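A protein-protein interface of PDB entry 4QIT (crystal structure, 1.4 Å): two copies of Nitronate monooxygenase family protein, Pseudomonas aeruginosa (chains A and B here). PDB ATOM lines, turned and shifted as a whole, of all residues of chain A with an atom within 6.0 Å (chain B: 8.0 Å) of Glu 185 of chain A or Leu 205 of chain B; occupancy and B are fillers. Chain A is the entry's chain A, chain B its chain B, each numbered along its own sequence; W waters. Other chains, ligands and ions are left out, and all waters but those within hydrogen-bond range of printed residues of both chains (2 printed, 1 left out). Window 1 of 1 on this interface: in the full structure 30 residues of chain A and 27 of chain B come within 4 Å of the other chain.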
ATOM      1  N   GLY A 183      -9.998  -7.141   6.082  1.00  0.00           N
ATOM      2  CA  GLY A 183      -9.688  -7.938   4.907  1.00  0.00           C
ATOM      3  C   GLY A 183      -9.624  -9.420   5.242  1.00  0.00           C
ATOM      4  O   GLY A 183      -9.556  -9.814   6.422  1.00  0.00           O
ATOM      5  N   ILE A 184      -9.607 -10.245   4.189  1.00  0.00           N
ATOM      6  CA  ILE A 184      -9.565 -11.694   4.340  1.00  0.00           C
ATOM      7  C   ILE A 184      -8.320 -12.144   5.116  1.00  0.00           C
ATOM      8  O   ILE A 184      -8.339 -13.183   5.774  1.00  0.00           O
ATOM      9  CB  ILE A 184      -9.676 -12.422   2.960  1.00  0.00           C
ATOM     10  CG1 ILE A 184     -10.109 -13.889   3.127  1.00  0.00           C
ATOM     11  CG2 ILE A 184      -8.368 -12.354   2.209  1.00  0.00           C
ATOM     12  CD1 ILE A 184     -11.407 -14.087   3.858  1.00  0.00           C
ATOM     13  N   GLU A 185      -7.268 -11.330   5.074  1.00  0.00           N
ATOM     14  CA  GLU A 185      -6.020 -11.614   5.790  1.00  0.00           C
ATOM     15  C   GLU A 185      -6.193 -11.723   7.295  1.00  0.00           C
ATOM     16  O   GLU A 185      -5.378 -12.360   7.974  1.00  0.00           O
ATOM     17  CB  GLU A 185      -5.008 -10.492   5.540  1.00  0.00           C
ATOM     18  CG  GLU A 185      -4.308 -10.519   4.192  1.00  0.00           C
ATOM     19  CD  GLU A 185      -4.986  -9.706   3.104  1.00  0.00           C
ATOM     20  OE1 GLU A 185      -6.234  -9.581   3.091  1.00  0.00           O
ATOM     21  OE2 GLU A 185      -4.254  -9.198   2.226  1.00  0.00           O
ATOM     22  N   ALA A 186      -7.214 -11.057   7.829  1.00  0.00           N
ATOM     23  CA  ALA A 186      -7.315 -10.870   9.276  1.00  0.00           C
ATOM     24  C   ALA A 186      -7.400 -12.160  10.049  1.00  0.00           C
ATOM     25  O   ALA A 186      -8.022 -13.136   9.605  1.00  0.00           O
ATOM     26  CB  ALA A 186      -8.497  -9.993   9.623  1.00  0.00           C
ATOM     27  N   GLY A 187      -6.795 -12.150  11.230  1.00  0.00           N
ATOM     28  CA  GLY A 187      -6.940 -13.248  12.163  1.00  0.00           C
ATOM     29  C   GLY A 187      -8.233 -13.185  12.958  1.00  0.00           C
ATOM     30  O   GLY A 187      -8.875 -12.138  13.062  1.00  0.00           O
ATOM     31  N   ARG A 190     -14.213 -13.635  11.376  1.00  0.00           N
ATOM     32  CA  ARG A 190     -14.566 -12.732  10.286  1.00  0.00           C
ATOM     33  C   ARG A 190     -15.761 -11.857  10.667  1.00  0.00           C
ATOM     34  O   ARG A 190     -16.731 -12.330  11.248  1.00  0.00           O
ATOM     35  CB  ARG A 190     -14.830 -13.502   8.996  1.00  0.00           C
ATOM     36  CG  ARG A 190     -13.526 -14.047   8.430  1.00  0.00           C
ATOM     37  CD  ARG A 190     -13.560 -14.448   6.980  1.00  0.00           C
ATOM     38  NE  ARG A 190     -14.181 -13.482   6.064  1.00  0.00           N
ATOM     39  CZ  ARG A 190     -13.699 -12.290   5.713  1.00  0.00           C
ATOM     40  NH1 ARG A 190     -12.574 -11.811   6.226  1.00  0.00           N
ATOM     41  NH2 ARG A 190     -14.367 -11.566   4.828  1.00  0.00           N
ATOM     42  N   ILE A 202     -13.065 -10.476   0.595  1.00  0.00           N
ATOM     43  CA  ILE A 202     -12.284  -9.447  -0.078  1.00  0.00           C
ATOM     44  C   ILE A 202     -10.972  -9.194   0.665  1.00  0.00           C
ATOM     45  O   ILE A 202     -10.958  -9.065   1.901  1.00  0.00           O
ATOM     46  CB  ILE A 202     -13.083  -8.133  -0.157  1.00  0.00           C
ATOM     47  CG1 ILE A 202     -14.442  -8.378  -0.823  1.00  0.00           C
ATOM     48  CG2 ILE A 202     -12.298  -7.069  -0.898  1.00  0.00           C
ATOM     49  CD1 ILE A 202     -15.353  -7.164  -0.803  1.00  0.00           C
ATOM     50  N   GLY A 203      -9.869  -9.153  -0.072  1.00  0.00           N
ATOM     51  CA  GLY A 203      -8.570  -8.917   0.536  1.00  0.00           C
ATOM     52  C   GLY A 203      -8.422  -7.481   0.993  1.00  0.00           C
ATOM     53  O   GLY A 203      -9.079  -6.575   0.461  1.00  0.00           O
ATOM     54  N   THR A 204      -7.531  -7.272   1.953  1.00  0.00           N
ATOM     55  CA  THR A 204      -7.311  -5.952   2.534  1.00  0.00           C
ATOM     56  C   THR A 204      -6.997  -4.869   1.487  1.00  0.00           C
ATOM     57  O   THR A 204      -7.543  -3.762   1.549  1.00  0.00           O
ATOM     58  CB  THR A 204      -6.191  -6.009   3.593  1.00  0.00           C
ATOM     59  OG1 THR A 204      -6.576  -6.888   4.648  1.00  0.00           O
ATOM     60  CG2 THR A 204      -5.917  -4.634   4.178  1.00  0.00           C
ATOM     61  N   LEU A 205      -6.125  -5.184   0.529  1.00  0.00           N
ATOM     62  CA  LEU A 205      -5.705  -4.189  -0.449  1.00  0.00           C
ATOM     63  C   LEU A 205      -6.895  -3.705  -1.272  1.00  0.00           C
ATOM     64  O   LEU A 205      -7.028  -2.503  -1.524  1.00  0.00           O
ATOM     65  CB  LEU A 205      -4.605  -4.746  -1.343  1.00  0.00           C
ATOM     66  CG  LEU A 205      -4.099  -3.760  -2.398  1.00  0.00           C
ATOM     67  CD1 LEU A 205      -2.580  -3.719  -2.400  1.00  0.00           C
ATOM     68  CD2 LEU A 205      -4.651  -4.166  -3.763  1.00  0.00           C
ATOM     69  N   ALA A 222      -7.592  -3.287   8.546  1.00  0.00           N
ATOM     70  CA  ALA A 222      -7.351  -4.414   9.445  1.00  0.00           C
ATOM     71  C   ALA A 222      -7.167  -5.687   8.643  1.00  0.00           C
ATOM     72  O   ALA A 222      -8.041  -6.080   7.863  1.00  0.00           O
ATOM     73  CB  ALA A 222      -8.497  -4.580  10.431  1.00  0.00           C
ATOM     74  N   GLY A 223      -6.036  -6.353   8.843  1.00  0.00           N
ATOM     75  CA  GLY A 223      -5.821  -7.654   8.225  1.00  0.00           C
ATOM     76  C   GLY A 223      -4.501  -7.758   7.493  1.00  0.00           C
ATOM     77  O   GLY A 223      -4.316  -7.217   6.404  1.00  0.00           O
ATOM     78  N   GLY A 224      -3.566  -8.472   8.116  1.00  0.00           N
ATOM     79  CA  GLY A 224      -2.292  -8.770   7.495  1.00  0.00           C
ATOM     80  C   GLY A 224      -1.194  -7.744   7.688  1.00  0.00           C
ATOM     81  O   GLY A 224      -0.092  -7.910   7.168  1.00  0.00           O
ATOM     82  N   ILE A 225      -1.480  -6.695   8.448  1.00  0.00           N
ATOM     83  CA  ILE A 225      -0.513  -5.618   8.659  1.00  0.00           C
ATOM     84  C   ILE A 225       0.369  -5.934   9.876  1.00  0.00           C
ATOM     85  O   ILE A 225      -0.138  -6.119  10.981  1.00  0.00           O
ATOM     86  CB  ILE A 225      -1.254  -4.287   8.818  1.00  0.00           C
ATOM     87  CG1 ILE A 225      -2.002  -3.978   7.512  1.00  0.00           C
ATOM     88  CG2 ILE A 225      -0.272  -3.163   9.168  1.00  0.00           C
ATOM     89  CD1 ILE A 225      -3.034  -2.862   7.633  1.00  0.00           C
ATOM     90  N   GLY A 230       3.647  -2.183   5.983  1.00  0.00           N
ATOM     91  CA  GLY A 230       2.219  -2.478   5.876  1.00  0.00           C
ATOM     92  C   GLY A 230       1.341  -1.285   6.231  1.00  0.00           C
ATOM     93  O   GLY A 230       0.324  -1.022   5.577  1.00  0.00           O
ATOM     94  N   ALA A 233       1.543   1.189   3.397  1.00  0.00           N
ATOM     95  CA  ALA A 233       0.748   0.722   2.260  1.00  0.00           C
ATOM     96  C   ALA A 233      -0.738   0.998   2.488  1.00  0.00           C
ATOM     97  O   ALA A 233      -1.434   1.463   1.581  1.00  0.00           O
ATOM     98  CB  ALA A 233       0.988  -0.767   2.000  1.00  0.00           C
ATOM     99  N   ALA A 234      -1.221   0.712   3.697  1.00  0.00           N
ATOM    100  CA  ALA A 234      -2.614   0.998   4.056  1.00  0.00           C
ATOM    101  C   ALA A 234      -2.936   2.478   3.874  1.00  0.00           C
ATOM    102  O   ALA A 234      -3.995   2.835   3.340  1.00  0.00           O
ATOM    103  CB  ALA A 234      -2.883   0.584   5.483  1.00  0.00           C
ATOM    104  N   LEU A 237      -3.383   3.467   0.348  1.00  0.00           N
ATOM    105  CA  LEU A 237      -4.675   3.015  -0.183  1.00  0.00           C
ATOM    106  C   LEU A 237      -5.822   3.941   0.222  1.00  0.00           C
ATOM    107  O   LEU A 237      -6.929   3.846  -0.313  1.00  0.00           O
ATOM    108  CB  LEU A 237      -4.973   1.587   0.268  1.00  0.00           C
ATOM    109  CG  LEU A 237      -4.017   0.539  -0.297  1.00  0.00           C
ATOM    110  CD1 LEU A 237      -4.266  -0.799   0.395  1.00  0.00           C
ATOM    111  CD2 LEU A 237      -4.181   0.404  -1.805  1.00  0.00           C
ATOM    112  N   THR A 272      -2.189 -20.256   7.778  1.00  0.00           N
ATOM    113  CA  THR A 272      -3.446 -20.098   8.506  1.00  0.00           C
ATOM    114  C   THR A 272      -4.599 -20.621   7.657  1.00  0.00           C
ATOM    115  O   THR A 272      -4.469 -20.800   6.445  1.00  0.00           O
ATOM    116  CB  THR A 272      -3.745 -18.630   8.888  1.00  0.00           C
ATOM    117  OG1 THR A 272      -4.007 -17.861   7.700  1.00  0.00           O
ATOM    118  CG2 THR A 272      -2.583 -18.009   9.670  1.00  0.00           C
ATOM    119  N   ARG A 284     -10.180 -17.214  11.453  1.00  0.00           N
ATOM    120  CA  ARG A 284      -8.878 -17.585  10.930  1.00  0.00           C
ATOM    121  C   ARG A 284      -7.850 -17.866  12.023  1.00  0.00           C
ATOM    122  O   ARG A 284      -7.618 -17.034  12.900  1.00  0.00           O
ATOM    123  CB  ARG A 284      -8.336 -16.491  10.012  1.00  0.00           C
ATOM    124  CG  ARG A 284      -6.944 -16.848   9.444  1.00  0.00           C
ATOM    125  CD  ARG A 284      -6.358 -15.755   8.528  1.00  0.00           C
ATOM    126  NE  ARG A 284      -7.227 -15.496   7.380  1.00  0.00           N
ATOM    127  CZ  ARG A 284      -7.381 -16.313   6.344  1.00  0.00           C
ATOM    128  NH1 ARG A 284      -6.716 -17.467   6.276  1.00  0.00           N
ATOM    129  NH2 ARG A 284      -8.231 -15.973   5.380  1.00  0.00           N
ATOM    130  N   ALA A 332      -4.700 -16.228  14.191  1.00  0.00           N
ATOM    131  CA  ALA A 332      -3.584 -15.558  13.546  1.00  0.00           C
ATOM    132  C   ALA A 332      -3.985 -15.149  12.137  1.00  0.00           C
ATOM    133  O   ALA A 332      -4.698 -15.886  11.461  1.00  0.00           O
ATOM    134  CB  ALA A 332      -2.358 -16.475  13.507  1.00  0.00           C
ATOM    135  N   GLY A 333      -3.519 -13.973  11.717  1.00  0.00           N
ATOM    136  CA  GLY A 333      -3.746 -13.463  10.373  1.00  0.00           C
ATOM    137  C   GLY A 333      -2.722 -13.982   9.377  1.00  0.00           C
ATOM    138  O   GLY A 333      -1.760 -14.675   9.747  1.00  0.00           O
ATOM    139  N   GLN A 334      -2.897 -13.612   8.115  1.00  0.00           N
ATOM    140  CA  GLN A 334      -2.057 -14.154   7.052  1.00  0.00           C
ATOM    141  C   GLN A 334      -0.645 -13.565   7.052  1.00  0.00           C
ATOM    142  O   GLN A 334       0.212 -14.032   6.306  1.00  0.00           O
ATOM    143  CB  GLN A 334      -2.739 -14.004   5.689  1.00  0.00           C
ATOM    144  CG  GLN A 334      -3.964 -14.903   5.532  1.00  0.00           C
ATOM    145  CD  GLN A 334      -4.606 -14.778   4.165  1.00  0.00           C
ATOM    146  OE1 GLN A 334      -4.546 -13.725   3.536  1.00  0.00           O
ATOM    147  NE2 GLN A 334      -5.204 -15.871   3.683  1.00  0.00           N
ATOM    148  N   GLY A 335      -0.391 -12.573   7.899  1.00  0.00           N
ATOM    149  CA  GLY A 335       0.964 -12.079   8.104  1.00  0.00           C
ATOM    150  C   GLY A 335       1.673 -12.725   9.282  1.00  0.00           C
ATOM    151  O   GLY A 335       2.708 -12.212   9.726  1.00  0.00           O
ATOM    152  N   ALA B 181       3.721 -12.168  -7.508  1.00  0.00           N
ATOM    153  CA  ALA B 181       2.937 -12.518  -6.320  1.00  0.00           C
ATOM    154  C   ALA B 181       1.464 -12.240  -6.565  1.00  0.00           C
ATOM    155  O   ALA B 181       1.037 -11.081  -6.552  1.00  0.00           O
ATOM    156  CB  ALA B 181       3.424 -11.710  -5.121  1.00  0.00           C
ATOM    157  N   GLY B 183      -2.218 -12.262  -5.399  1.00  0.00           N
ATOM    158  CA  GLY B 183      -3.077 -12.293  -4.240  1.00  0.00           C
ATOM    159  C   GLY B 183      -4.476 -12.763  -4.580  1.00  0.00           C
ATOM    160  O   GLY B 183      -4.867 -12.856  -5.755  1.00  0.00           O
ATOM    161  N   ILE B 184      -5.255 -13.020  -3.538  1.00  0.00           N
ATOM    162  CA  ILE B 184      -6.618 -13.521  -3.702  1.00  0.00           C
ATOM    163  C   ILE B 184      -7.503 -12.529  -4.472  1.00  0.00           C
ATOM    164  O   ILE B 184      -8.449 -12.939  -5.139  1.00  0.00           O
ATOM    165  CB  ILE B 184      -7.251 -13.901  -2.325  1.00  0.00           C
ATOM    166  CG1 ILE B 184      -8.458 -14.831  -2.513  1.00  0.00           C
ATOM    167  CG2 ILE B 184      -7.658 -12.658  -1.552  1.00  0.00           C
ATOM    168  CD1 ILE B 184      -8.186 -16.115  -3.284  1.00  0.00           C
ATOM    169  N   GLU B 185      -7.151 -11.244  -4.425  1.00  0.00           N
ATOM    170  CA  GLU B 185      -7.860 -10.208  -5.177  1.00  0.00           C
ATOM    171  C   GLU B 185      -7.861 -10.439  -6.685  1.00  0.00           C
ATOM    172  O   GLU B 185      -8.743  -9.945  -7.387  1.00  0.00           O
ATOM    173  CB  GLU B 185      -7.227  -8.834  -4.922  1.00  0.00           C
ATOM    174  CG  GLU B 185      -7.546  -8.235  -3.563  1.00  0.00           C
ATOM    175  CD  GLU B 185      -6.544  -8.568  -2.486  1.00  0.00           C
ATOM    176  OE1 GLU B 185      -5.929  -9.669  -2.521  1.00  0.00           O
ATOM    177  OE2 GLU B 185      -6.383  -7.707  -1.586  1.00  0.00           O
ATOM    178  N   ALA B 201      -5.191 -19.145  -0.318  1.00  0.00           N
ATOM    179  CA  ALA B 201      -5.991 -17.940  -0.601  1.00  0.00           C
ATOM    180  C   ALA B 201      -5.495 -16.717   0.162  1.00  0.00           C
ATOM    181  O   ALA B 201      -6.241 -16.080   0.914  1.00  0.00           O
ATOM    182  CB  ALA B 201      -7.481 -18.205  -0.312  1.00  0.00           C
ATOM    183  N   ILE B 202      -4.218 -16.405  -0.031  1.00  0.00           N
ATOM    184  CA  ILE B 202      -3.576 -15.298   0.667  1.00  0.00           C
ATOM    185  C   ILE B 202      -3.830 -13.973  -0.066  1.00  0.00           C
ATOM    186  O   ILE B 202      -3.656 -13.883  -1.285  1.00  0.00           O
ATOM    187  CB  ILE B 202      -2.052 -15.534   0.786  1.00  0.00           C
ATOM    188  CG1 ILE B 202      -1.782 -16.859   1.505  1.00  0.00           C
ATOM    189  CG2 ILE B 202      -1.399 -14.361   1.516  1.00  0.00           C
ATOM    190  CD1 ILE B 202      -0.318 -17.296   1.506  1.00  0.00           C
ATOM    191  N   GLY B 203      -4.236 -12.950   0.677  1.00  0.00           N
ATOM    192  CA  GLY B 203      -4.477 -11.638   0.096  1.00  0.00           C
ATOM    193  C   GLY B 203      -3.197 -10.964  -0.371  1.00  0.00           C
ATOM    194  O   GLY B 203      -2.103 -11.267   0.123  1.00  0.00           O
ATOM    195  N   THR B 204      -3.340 -10.037  -1.316  1.00  0.00           N
ATOM    196  CA  THR B 204      -2.206  -9.345  -1.901  1.00  0.00           C
ATOM    197  C   THR B 204      -1.331  -8.665  -0.854  1.00  0.00           C
ATOM    198  O   THR B 204      -0.096  -8.778  -0.894  1.00  0.00           O
ATOM    199  CB  THR B 204      -2.679  -8.323  -2.955  1.00  0.00           C
ATOM    200  OG1 THR B 204      -3.348  -9.020  -4.009  1.00  0.00           O
ATOM    201  CG2 THR B 204      -1.504  -7.566  -3.535  1.00  0.00           C
ATOM    202  N   LEU B 205      -1.962  -7.973   0.087  1.00  0.00           N
ATOM    203  CA  LEU B 205      -1.210  -7.206   1.084  1.00  0.00           C
ATOM    204  C   LEU B 205      -0.304  -8.112   1.916  1.00  0.00           C
ATOM    205  O   LEU B 205       0.856  -7.771   2.153  1.00  0.00           O
ATOM    206  CB  LEU B 205      -2.141  -6.375   1.976  1.00  0.00           C
ATOM    207  CG  LEU B 205      -1.415  -5.520   3.023  1.00  0.00           C
ATOM    208  CD1 LEU B 205      -1.923  -4.084   3.017  1.00  0.00           C
ATOM    209  CD2 LEU B 205      -1.526  -6.149   4.427  1.00  0.00           C
ATOM    210  N   ALA B 206      -0.816  -9.259   2.362  1.00  0.00           N
ATOM    211  CA  ALA B 206       0.032 -10.217   3.078  1.00  0.00           C
ATOM    212  C   ALA B 206       1.066 -10.867   2.163  1.00  0.00           C
ATOM    213  O   ALA B 206       2.242 -10.967   2.517  1.00  0.00           O
ATOM    214  CB  ALA B 206      -0.799 -11.294   3.766  1.00  0.00           C
ATOM    215  N   LEU B 207       0.635 -11.324   0.990  1.00  0.00           N
ATOM    216  CA  LEU B 207       1.521 -12.112   0.128  1.00  0.00           C
ATOM    217  C   LEU B 207       2.729 -11.310  -0.342  1.00  0.00           C
ATOM    218  O   LEU B 207       3.866 -11.792  -0.285  1.00  0.00           O
ATOM    219  CB  LEU B 207       0.771 -12.668  -1.082  1.00  0.00           C
ATOM    220  CG  LEU B 207       1.614 -13.579  -1.992  1.00  0.00           C
ATOM    221  CD1 LEU B 207       2.089 -14.844  -1.251  1.00  0.00           C
ATOM    222  CD2 LEU B 207       0.835 -13.946  -3.249  1.00  0.00           C
ATOM    223  N   VAL B 208       2.485 -10.102  -0.830  1.00  0.00           N
ATOM    224  CA  VAL B 208       3.576  -9.265  -1.316  1.00  0.00           C
ATOM    225  C   VAL B 208       4.576  -9.002  -0.187  1.00  0.00           C
ATOM    226  O   VAL B 208       5.794  -9.113  -0.384  1.00  0.00           O
ATOM    227  CB  VAL B 208       3.047  -7.937  -1.922  1.00  0.00           C
ATOM    228  CG1 VAL B 208       4.205  -7.008  -2.281  1.00  0.00           C
ATOM    229  CG2 VAL B 208       2.199  -8.233  -3.153  1.00  0.00           C
ATOM    230  N   ARG B 209       4.075  -8.670   0.996  1.00  0.00           N
ATOM    231  CA  ARG B 209       4.962  -8.400   2.129  1.00  0.00           C
ATOM    232  C   ARG B 209       5.767  -9.643   2.493  1.00  0.00           C
ATOM    233  O   ARG B 209       6.970  -9.570   2.749  1.00  0.00           O
ATOM    234  CB  ARG B 209       4.177  -7.915   3.341  1.00  0.00           C
ATOM    235  CG  ARG B 209       5.063  -7.354   4.460  1.00  0.00           C
ATOM    236  CD  ARG B 209       5.642  -5.954   4.135  1.00  0.00           C
ATOM    237  NE  ARG B 209       6.833  -5.697   4.940  1.00  0.00           N
ATOM    238  CZ  ARG B 209       8.087  -5.769   4.497  1.00  0.00           C
ATOM    239  NH1 ARG B 209       8.350  -6.009   3.217  1.00  0.00           N
ATOM    240  NH2 ARG B 209       9.090  -5.533   5.336  1.00  0.00           N
ATOM    241  N   LEU B 210       5.114 -10.798   2.496  1.00  0.00           N
ATOM    242  CA  LEU B 210       5.801 -12.036   2.836  1.00  0.00           C
ATOM    243  C   LEU B 210       6.959 -12.320   1.885  1.00  0.00           C
ATOM    244  O   LEU B 210       8.058 -12.684   2.323  1.00  0.00           O
ATOM    245  CB  LEU B 210       4.807 -13.204   2.841  1.00  0.00           C
ATOM    246  CG  LEU B 210       3.830 -13.208   4.021  1.00  0.00           C
ATOM    247  CD1 LEU B 210       2.645 -14.095   3.708  1.00  0.00           C
ATOM    248  CD2 LEU B 210       4.544 -13.684   5.287  1.00  0.00           C
ATOM    249  N   LEU B 211       6.718 -12.148   0.590  1.00  0.00           N
ATOM    250  CA  LEU B 211       7.731 -12.456  -0.413  1.00  0.00           C
ATOM    251  C   LEU B 211       8.847 -11.418  -0.415  1.00  0.00           C
ATOM    252  O   LEU B 211      10.022 -11.768  -0.572  1.00  0.00           O
ATOM    253  CB  LEU B 211       7.105 -12.583  -1.807  1.00  0.00           C
ATOM    254  CG  LEU B 211       6.674 -13.995  -2.240  1.00  0.00           C
ATOM    255  CD1 LEU B 211       6.024 -14.806  -1.128  1.00  0.00           C
ATOM    256  CD2 LEU B 211       5.803 -13.988  -3.481  1.00  0.00           C
ATOM    257  N   ALA B 221       3.803  -7.356  -7.716  1.00  0.00           N
ATOM    258  CA  ALA B 221       2.497  -7.471  -7.045  1.00  0.00           C
ATOM    259  C   ALA B 221       1.351  -7.563  -8.044  1.00  0.00           C
ATOM    260  O   ALA B 221       1.209  -6.706  -8.912  1.00  0.00           O
ATOM    261  CB  ALA B 221       2.276  -6.275  -6.142  1.00  0.00           C
ATOM    262  N   ALA B 222       0.517  -8.587  -7.902  1.00  0.00           N
ATOM    263  CA  ALA B 222      -0.628  -8.773  -8.786  1.00  0.00           C
ATOM    264  C   ALA B 222      -1.888  -9.079  -7.986  1.00  0.00           C
ATOM    265  O   ALA B 222      -1.920 -10.033  -7.202  1.00  0.00           O
ATOM    266  CB  ALA B 222      -0.347  -9.901  -9.772  1.00  0.00           C
ATOM    267  N   GLY B 223      -2.931  -8.289  -8.194  1.00  0.00           N
ATOM    268  CA  GLY B 223      -4.242  -8.608  -7.641  1.00  0.00           C
ATOM    269  C   GLY B 223      -4.866  -7.429  -6.929  1.00  0.00           C
ATOM    270  O   GLY B 223      -4.452  -7.069  -5.817  1.00  0.00           O
ATOM    271  N   ALA B 233       1.067   1.560  -2.898  1.00  0.00           N
ATOM    272  CA  ALA B 233       0.894   0.667  -1.756  1.00  0.00           C
ATOM    273  C   ALA B 233       1.743  -0.587  -1.941  1.00  0.00           C
ATOM    274  O   ALA B 233       2.427  -1.039  -1.006  1.00  0.00           O
ATOM    275  CB  ALA B 233      -0.577   0.297  -1.601  1.00  0.00           C
ATOM    276  N   ALA B 234       1.706  -1.143  -3.153  1.00  0.00           N
ATOM    277  CA  ALA B 234       2.499  -2.325  -3.476  1.00  0.00           C
ATOM    278  C   ALA B 234       3.988  -2.066  -3.307  1.00  0.00           C
ATOM    279  O   ALA B 234       4.713  -2.896  -2.733  1.00  0.00           O
ATOM    280  CB  ALA B 234       2.203  -2.789  -4.886  1.00  0.00           C
ATOM    281  N   LEU B 237       4.986  -2.073   0.252  1.00  0.00           N
ATOM    282  CA  LEU B 237       5.085  -3.442   0.764  1.00  0.00           C
ATOM    283  C   LEU B 237       6.380  -4.129   0.350  1.00  0.00           C
ATOM    284  O   LEU B 237       6.709  -5.204   0.865  1.00  0.00           O
ATOM    285  CB  LEU B 237       3.899  -4.276   0.285  1.00  0.00           C
ATOM    286  CG  LEU B 237       2.535  -3.831   0.813  1.00  0.00           C
ATOM    287  CD1 LEU B 237       1.454  -4.594   0.057  1.00  0.00           C
ATOM    288  CD2 LEU B 237       2.387  -4.031   2.317  1.00  0.00           C
ATOM    289  N   GLN B 334     -10.848  -8.123  -7.553  1.00  0.00           N
ATOM    290  CA  GLN B 334     -11.695  -7.530  -6.522  1.00  0.00           C
ATOM    291  C   GLN B 334     -11.688  -5.999  -6.520  1.00  0.00           C
ATOM    292  O   GLN B 334     -12.427  -5.386  -5.756  1.00  0.00           O
ATOM    293  CB  GLN B 334     -11.339  -8.089  -5.135  1.00  0.00           C
ATOM    294  CG  GLN B 334     -11.707  -9.576  -4.971  1.00  0.00           C
ATOM    295  CD  GLN B 334     -11.404 -10.119  -3.585  1.00  0.00           C
ATOM    296  OE1 GLN B 334     -10.440  -9.702  -2.941  1.00  0.00           O
ATOM    297  NE2 GLN B 334     -12.226 -11.047  -3.117  1.00  0.00           N
HETATM  298  O   HOH W   1       1.698  -7.198   5.156  1.00  0.00           O
HETATM  299  O   HOH W   2      -8.325 -17.022   2.599  1.00  0.00           O
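The backbone NH (N) of Leu 205 of chain A is in hydrogen-bond range of the side-chain carboxylate (OE2) of Glu 185 of chain B (3.3 Å). The backbone NH (N) of Gly 203 of chain B lies within hydrogen-bond range of the side-chain amide oxygen (OE1) of Gln 334 of chain A (3.0 Å). The side-chain amide nitrogen (NE2) of Gln 334 of chain A lies within hydrogen-bond range of the backbone carbonyl oxygen (O) of Ala 201 of chain B, 3.0 Å away. N of Gly 203 of chain A is in hydrogen-bond range of OE1 of Gln 334 of chain B (3.0 Å). The side-chain carboxylate of Glu 185 of chain A sits at hydrogen-bond distance from the backbone NH of Leu 205 of chain B, at 3.4 Å. The backbone NH of Ala 206 of chain B sits at hydrogen-bond distance from the side-chain carboxylate of Glu 185 of chain A.
Glu 185 of chain A touches Gly 203 of chain B (OE2 to CA, 3.2 Å). Thr 204 of chain B touches Glu 185 of chain A (N to OE2, 3.8 Å). CA of Gly 203 of chain A touches OE2 of Glu 185 of chain B, 3.3 Å away. Gly 223 of chain A touches Leu 205 of chain B. Gly 230 of chain A touches Leu 237 of chain B. CB of Ala 233 of chain B touches CD2 of Leu 237 of chain A (3.6 Å). Ile 202 of chain B touches Gln 334 of chain A (CA to OE1, 3.4 Å).
Water W1 lies within hydrogen-bond range of O of Gly 224 of chain A (2.8 Å) and O of Leu 205 of chain B (3.2 Å). Water W2 lies within hydrogen-bond range of O of Ala 201 of chain B (2.8 Å), NH2 of Arg 284 of chain A (3.0 Å) and NE2 of Gln 334 of chain A (3.5 Å).
Glu 185 of chain A touches Gly 203 of chain B, and with the chains exchanged Gly 203 of chain A touches Glu 185 of chain B. Glu 185 of chain A touches Thr 204 of chain B, and with the chains exchanged Thr 204 of chain A touches Glu 185 of chain B. Leu 205 of chain A touches Gly 223 of chain B, and with the chains exchanged Gly 223 of chain A touches Leu 205 of chain B.
The backbone NH of Ile 184 of chain A sits at hydrogen-bond distance from the backbone carbonyl oxygen of Ile 202 of chain A, at 2.9 Å. The side-chain carboxylate (OE1) of Glu 185 of chain A is in hydrogen-bond range of the backbone NH (N) of Thr 204 of chain A (2.9 Å). The backbone NH of Gln 334 of chain A is in hydrogen-bond range of the backbone carbonyl oxygen of Glu 185 of chain A, 2.8 Å away.
Printed residues of chain B that touch a printed residue of chain A: Ile 184, Glu 185, Ala 201, Ile 202, Gly 203, Thr 204, Leu 205, Ala 206, Leu 210, Gly 223, Ala 233, Leu 237 and Gln 334. Hydrophobic or aromatic side chains of chain B that line the printed part of chain A: Ile 184, Ile 202, Leu 205, Ala 206, Leu 210, Ala 233 and Leu 237. Hydrophobic or aromatic side chains of chain A that line the printed part of chain B: Ile 184, Ile 202, Leu 205, Ile 225, Ala 233 and Leu 237. Among the printed residues, 23 pairs touch across the chains.
Glu 185 of chain A touches four residues of chain B. Leu 205 of chain B touches just these residues of chain A: Glu 185 (3.4 Å), Gly 223 (3.6 Å), Gly 224 (3.6 Å) and Ile 225 (3.8 Å). No residue of chain B comes within 4 Å of Ala 186 of chain A. Gly 224 of chain A touches one residue of chain B. Printed residues of chain A within 4 Å of Ile 184 of chain B: Ile 184. Of the printed residues of chain A, Thr 204 of chain B touches Glu 185. Of the printed residues of chain B, Leu 205 of chain A touches Glu 185 (3.3 Å) and Gly 223 (3.6 Å). Printed residues of chain B within 4 Å of Gly 223 of chain A: Leu 205 (3.6 Å). Of the printed residues of chain A, Leu 237 of chain B touches Gly 230 and Ala 233. The nearest residue of chain A that does not touch Leu 205 of chain B is Thr 204 of chain A (4.2 Å). The nearest printed residue of chain B that does not touch Gly 223 of chain A is Ala 206 of chain B (5.7 Å).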
